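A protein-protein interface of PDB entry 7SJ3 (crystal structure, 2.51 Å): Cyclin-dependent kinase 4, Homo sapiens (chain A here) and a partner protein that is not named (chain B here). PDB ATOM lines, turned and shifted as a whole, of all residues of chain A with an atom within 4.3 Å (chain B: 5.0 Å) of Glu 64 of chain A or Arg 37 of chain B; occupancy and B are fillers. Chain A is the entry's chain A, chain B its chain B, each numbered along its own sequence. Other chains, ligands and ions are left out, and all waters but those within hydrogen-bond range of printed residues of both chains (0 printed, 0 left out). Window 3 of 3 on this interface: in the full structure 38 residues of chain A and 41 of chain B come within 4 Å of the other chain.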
ATOM      1  N   LEU A  60     -30.517 -10.433   1.804  1.00  0.00           N
ATOM      2  CA  LEU A  60     -30.278 -11.273   0.636  1.00  0.00           C
ATOM      3  C   LEU A  60     -30.445 -10.486  -0.658  1.00  0.00           C
ATOM      4  O   LEU A  60     -29.673 -10.665  -1.609  1.00  0.00           O
ATOM      5  CB  LEU A  60     -31.211 -12.484   0.667  1.00  0.00           C
ATOM      6  CG  LEU A  60     -30.891 -13.492   1.773  1.00  0.00           C
ATOM      7  CD1 LEU A  60     -32.019 -14.483   1.943  1.00  0.00           C
ATOM      8  CD2 LEU A  60     -29.589 -14.216   1.475  1.00  0.00           C
ATOM      9  N   ARG A  61     -31.442  -9.598  -0.707  1.00  0.00           N
ATOM     10  CA  ARG A  61     -31.641  -8.784  -1.903  1.00  0.00           C
ATOM     11  C   ARG A  61     -30.449  -7.862  -2.130  1.00  0.00           C
ATOM     12  O   ARG A  61     -30.062  -7.611  -3.277  1.00  0.00           O
ATOM     13  CB  ARG A  61     -32.953  -7.999  -1.806  1.00  0.00           C
ATOM     14  CG  ARG A  61     -34.152  -8.852  -2.235  1.00  0.00           C
ATOM     15  CD  ARG A  61     -34.286  -8.991  -3.742  1.00  0.00           C
ATOM     16  NE  ARG A  61     -35.637  -9.383  -4.130  1.00  0.00           N
ATOM     17  CZ  ARG A  61     -35.941 -10.534  -4.731  1.00  0.00           C
ATOM     18  NH1 ARG A  61     -34.988 -11.413  -5.022  1.00  0.00           N
ATOM     19  NH2 ARG A  61     -37.202 -10.802  -5.053  1.00  0.00           N
ATOM     20  N   ARG A  62     -29.869  -7.321  -1.051  1.00  0.00           N
ATOM     21  CA  ARG A  62     -28.683  -6.485  -1.206  1.00  0.00           C
ATOM     22  C   ARG A  62     -27.503  -7.314  -1.699  1.00  0.00           C
ATOM     23  O   ARG A  62     -26.730  -6.861  -2.552  1.00  0.00           O
ATOM     24  CB  ARG A  62     -28.332  -5.801   0.122  1.00  0.00           C
ATOM     25  CG  ARG A  62     -27.034  -4.988   0.071  1.00  0.00           C
ATOM     26  CD  ARG A  62     -26.470  -4.699   1.461  1.00  0.00           C
ATOM     27  NE  ARG A  62     -26.982  -3.467   2.054  1.00  0.00           N
ATOM     28  CZ  ARG A  62     -26.232  -2.417   2.375  1.00  0.00           C
ATOM     29  NH1 ARG A  62     -24.922  -2.443   2.182  1.00  0.00           N
ATOM     30  NH2 ARG A  62     -26.791  -1.343   2.911  1.00  0.00           N
ATOM     31  N   LEU A  63     -27.337  -8.521  -1.151  1.00  0.00           N
ATOM     32  CA  LEU A  63     -26.238  -9.399  -1.539  1.00  0.00           C
ATOM     33  C   LEU A  63     -26.426 -10.019  -2.916  1.00  0.00           C
ATOM     34  O   LEU A  63     -25.437 -10.410  -3.545  1.00  0.00           O
ATOM     35  CB  LEU A  63     -26.065 -10.524  -0.521  1.00  0.00           C
ATOM     36  CG  LEU A  63     -25.672 -10.102   0.886  1.00  0.00           C
ATOM     37  CD1 LEU A  63     -25.738 -11.294   1.818  1.00  0.00           C
ATOM     38  CD2 LEU A  63     -24.276  -9.508   0.847  1.00  0.00           C
ATOM     39  N   GLU A  64     -27.663 -10.097  -3.409  1.00  0.00           N
ATOM     40  CA  GLU A  64     -27.911 -10.706  -4.710  1.00  0.00           C
ATOM     41  C   GLU A  64     -27.242  -9.941  -5.839  1.00  0.00           C
ATOM     42  O   GLU A  64     -26.959 -10.525  -6.892  1.00  0.00           O
ATOM     43  CB  GLU A  64     -29.425 -10.797  -4.935  1.00  0.00           C
ATOM     44  CG  GLU A  64     -29.882 -10.733  -6.383  1.00  0.00           C
ATOM     45  CD  GLU A  64     -31.221 -10.038  -6.544  1.00  0.00           C
ATOM     46  OE1 GLU A  64     -32.232 -10.552  -6.019  1.00  0.00           O
ATOM     47  OE2 GLU A  64     -31.255  -8.968  -7.188  1.00  0.00           O
ATOM     48  N   ALA A  65     -26.901  -8.674  -5.614  1.00  0.00           N
ATOM     49  CA  ALA A  65     -26.256  -7.892  -6.658  1.00  0.00           C
ATOM     50  C   ALA A  65     -24.856  -8.399  -6.977  1.00  0.00           C
ATOM     51  O   ALA A  65     -24.329  -8.082  -8.047  1.00  0.00           O
ATOM     52  CB  ALA A  65     -26.201  -6.418  -6.251  1.00  0.00           C
ATOM     53  N   PHE A  66     -24.253  -9.201  -6.093  1.00  0.00           N
ATOM     54  CA  PHE A  66     -22.892  -9.677  -6.306  1.00  0.00           C
ATOM     55  C   PHE A  66     -22.799 -11.108  -6.816  1.00  0.00           C
ATOM     56  O   PHE A  66     -21.774 -11.457  -7.416  1.00  0.00           O
ATOM     57  CB  PHE A  66     -22.086  -9.564  -5.007  1.00  0.00           C
ATOM     58  CG  PHE A  66     -21.956  -8.158  -4.489  1.00  0.00           C
ATOM     59  CD1 PHE A  66     -20.978  -7.313  -4.992  1.00  0.00           C
ATOM     60  CD2 PHE A  66     -22.810  -7.679  -3.508  1.00  0.00           C
ATOM     61  CE1 PHE A  66     -20.846  -6.019  -4.522  1.00  0.00           C
ATOM     62  CE2 PHE A  66     -22.688  -6.382  -3.035  1.00  0.00           C
ATOM     63  CZ  PHE A  66     -21.701  -5.552  -3.542  1.00  0.00           C
ATOM     64  N   GLU A  67     -23.813 -11.945  -6.594  1.00  0.00           N
ATOM     65  CA  GLU A  67     -23.779 -13.344  -7.033  1.00  0.00           C
ATOM     66  C   GLU A  67     -22.546 -14.079  -6.504  1.00  0.00           C
ATOM     67  O   GLU A  67     -21.862 -14.797  -7.236  1.00  0.00           O
ATOM     68  CB  GLU A  67     -23.871 -13.456  -8.557  1.00  0.00           C
ATOM     69  CG  GLU A  67     -25.002 -12.656  -9.186  1.00  0.00           C
ATOM     70  CD  GLU A  67     -25.114 -12.877 -10.686  1.00  0.00           C
ATOM     71  OE1 GLU A  67     -24.135 -12.590 -11.410  1.00  0.00           O
ATOM     72  OE2 GLU A  67     -26.181 -13.347 -11.138  1.00  0.00           O
ATOM     73  N   LEU B  34     -22.452  -0.015  -4.267  1.00  0.00           N
ATOM     74  CA  LEU B  34     -23.858  -0.365  -4.101  1.00  0.00           C
ATOM     75  C   LEU B  34     -24.792   0.831  -4.235  1.00  0.00           C
ATOM     76  O   LEU B  34     -25.962   0.651  -4.581  1.00  0.00           O
ATOM     77  CB  LEU B  34     -24.092  -1.002  -2.730  1.00  0.00           C
ATOM     78  CG  LEU B  34     -23.900  -2.501  -2.549  1.00  0.00           C
ATOM     79  CD1 LEU B  34     -23.988  -2.840  -1.073  1.00  0.00           C
ATOM     80  CD2 LEU B  34     -24.949  -3.265  -3.347  1.00  0.00           C
ATOM     81  N   GLU B  35     -24.309   2.045  -3.959  1.00  0.00           N
ATOM     82  CA  GLU B  35     -25.216   3.156  -3.682  1.00  0.00           C
ATOM     83  C   GLU B  35     -26.083   3.491  -4.894  1.00  0.00           C
ATOM     84  O   GLU B  35     -27.275   3.789  -4.747  1.00  0.00           O
ATOM     85  CB  GLU B  35     -24.434   4.381  -3.185  1.00  0.00           C
ATOM     86  CG  GLU B  35     -23.423   4.981  -4.144  1.00  0.00           C
ATOM     87  CD  GLU B  35     -22.866   6.319  -3.650  1.00  0.00           C
ATOM     88  OE1 GLU B  35     -23.406   6.874  -2.666  1.00  0.00           O
ATOM     89  OE2 GLU B  35     -21.883   6.816  -4.243  1.00  0.00           O
ATOM     90  N   GLU B  36     -25.519   3.425  -6.101  1.00  0.00           N
ATOM     91  CA  GLU B  36     -26.298   3.828  -7.267  1.00  0.00           C
ATOM     92  C   GLU B  36     -27.494   2.916  -7.490  1.00  0.00           C
ATOM     93  O   GLU B  36     -28.480   3.337  -8.108  1.00  0.00           O
ATOM     94  CB  GLU B  36     -25.410   3.842  -8.514  1.00  0.00           C
ATOM     95  CG  GLU B  36     -24.344   4.929  -8.508  1.00  0.00           C
ATOM     96  CD  GLU B  36     -24.918   6.315  -8.746  1.00  0.00           C
ATOM     97  OE1 GLU B  36     -26.076   6.413  -9.211  1.00  0.00           O
ATOM     98  OE2 GLU B  36     -24.213   7.310  -8.472  1.00  0.00           O
ATOM     99  N   ARG B  37     -27.432   1.685  -6.979  1.00  0.00           N
ATOM    100  CA  ARG B  37     -28.551   0.757  -7.085  1.00  0.00           C
ATOM    101  C   ARG B  37     -29.788   1.295  -6.370  1.00  0.00           C
ATOM    102  O   ARG B  37     -30.919   0.983  -6.760  1.00  0.00           O
ATOM    103  CB  ARG B  37     -28.124  -0.614  -6.551  1.00  0.00           C
ATOM    104  CG  ARG B  37     -29.224  -1.611  -6.225  1.00  0.00           C
ATOM    105  CD  ARG B  37     -28.615  -2.853  -5.576  1.00  0.00           C
ATOM    106  NE  ARG B  37     -29.607  -3.873  -5.255  1.00  0.00           N
ATOM    107  CZ  ARG B  37     -29.866  -4.922  -6.033  1.00  0.00           C
ATOM    108  NH1 ARG B  37     -29.210  -5.082  -7.175  1.00  0.00           N
ATOM    109  NH2 ARG B  37     -30.783  -5.812  -5.677  1.00  0.00           N
ATOM    110  N   TYR B  38     -29.600   2.099  -5.325  1.00  0.00           N
ATOM    111  CA  TYR B  38     -30.711   2.581  -4.522  1.00  0.00           C
ATOM    112  C   TYR B  38     -31.069   4.036  -4.805  1.00  0.00           C
ATOM    113  O   TYR B  38     -31.880   4.616  -4.076  1.00  0.00           O
ATOM    114  CB  TYR B  38     -30.405   2.360  -3.039  1.00  0.00           C
ATOM    115  CG  TYR B  38     -30.221   0.882  -2.764  1.00  0.00           C
ATOM    116  CD1 TYR B  38     -31.320   0.039  -2.639  1.00  0.00           C
ATOM    117  CD2 TYR B  38     -28.952   0.326  -2.657  1.00  0.00           C
ATOM    118  CE1 TYR B  38     -31.164  -1.308  -2.406  1.00  0.00           C
ATOM    119  CE2 TYR B  38     -28.786  -1.031  -2.424  1.00  0.00           C
ATOM    120  CZ  TYR B  38     -29.896  -1.841  -2.298  1.00  0.00           C
ATOM    121  OH  TYR B  38     -29.741  -3.190  -2.066  1.00  0.00           O
ATOM    122  N   VAL B  39     -30.536   4.619  -5.871  1.00  0.00           N
ATOM    123  CA  VAL B  39     -30.905   5.984  -6.239  1.00  0.00           C
ATOM    124  C   VAL B  39     -32.176   5.925  -7.078  1.00  0.00           C
ATOM    125  O   VAL B  39     -32.231   5.174  -8.063  1.00  0.00           O
ATOM    126  CB  VAL B  39     -29.772   6.694  -6.992  1.00  0.00           C
ATOM    127  CG1 VAL B  39     -30.267   8.011  -7.574  1.00  0.00           C
ATOM    128  CG2 VAL B  39     -28.580   6.924  -6.068  1.00  0.00           C
ATOM    129  N   ASP B 151     -36.496  -4.914  -1.530  1.00  0.00           N
ATOM    130  CA  ASP B 151     -35.100  -4.473  -1.529  1.00  0.00           C
ATOM    131  C   ASP B 151     -34.976  -3.237  -0.638  1.00  0.00           C
ATOM    132  O   ASP B 151     -34.802  -2.104  -1.091  1.00  0.00           O
ATOM    133  CB  ASP B 151     -34.625  -4.202  -2.951  1.00  0.00           C
ATOM    134  CG  ASP B 151     -33.112  -4.209  -3.074  1.00  0.00           C
ATOM    135  OD1 ASP B 151     -32.429  -4.444  -2.051  1.00  0.00           O
ATOM    136  OD2 ASP B 151     -32.600  -3.976  -4.191  1.00  0.00           O
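O of Arg 61 of chain A lies within hydrogen-bond range of NH2 of Arg 37 of chain B, at 3.1 Å. The side-chain carboxylate (OE2) of Glu 64 of chain A is in salt-bridge range of the guanidinium group (NH2) of Arg 37 of chain B.
NH1 of Arg 61 of chain A is in salt-bridge range of OE1 of Glu 64 of chain A, 3.1 Å away. The guanidinium group of Arg 37 of chain B lies within hydrogen-bond range of the side-chain hydroxyl of Tyr 38 of chain B. NH2 of Arg 37 of chain B lies within salt-bridge range of OD2 of Asp 151 of chain B (3.0 Å). The side-chain hydroxyl of Tyr 38 of chain B lies within hydrogen-bond range of the side-chain carboxylate of Asp 151 of chain B.
Asp 151 of chain B touches Arg 61 of chain A. Leu 34 of chain B touches Arg 62 of chain A. CA of Arg 62 of chain A touches OH of Tyr 38 of chain B (3.6 Å). OD1 of Asp 151 of chain B touches N of Arg 62 of chain A (3.98 Å). Ala 65 of chain A touches Arg 37 of chain B (CB to NH1, 3.4 Å). CD2 of Leu 34 of chain B touches CE2 of Phe 66 of chain A, 3.9 Å away.
Of the printed residues of chain B, Arg 61 of chain A touches Arg 37 (3.1 Å) and Asp 151 (3.6 Å). Printed residues of chain B within 4 Å of Arg 62 of chain A: Leu 34 (3.4 Å), Tyr 38 (3.6 Å) and Asp 151 (3.98 Å). Glu 64 of chain A touches just one residue of chain B: Arg 37. Printed residues of chain B within 4 Å of Ala 65 of chain A: Arg 37. Of the printed residues of chain A, Leu 34 of chain B touches Arg 62 (3.4 Å) and Phe 66 (3.9 Å). Printed residues of chain A within 4 Å of Arg 37 of chain B: Arg 61 (3.1 Å), Glu 64 (3.5 Å) and Ala 65 (3.4 Å). Printed residues of chain A within 4 Å of Asp 151 of chain B: Arg 61 and Arg 62. The nearest printed residue of chain A that does not touch Arg 37 of chain B is Arg 62 of chain A (4.9 Å).
Hydrophobic or aromatic side chains of chain B that line the printed part of chain A: Leu 34 and Tyr 38. Hydrophobic or aromatic side chains of chain A that line the printed part of chain B: Ala 65 and Phe 66. Among the printed residues, 8 pairs touch across the chains.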
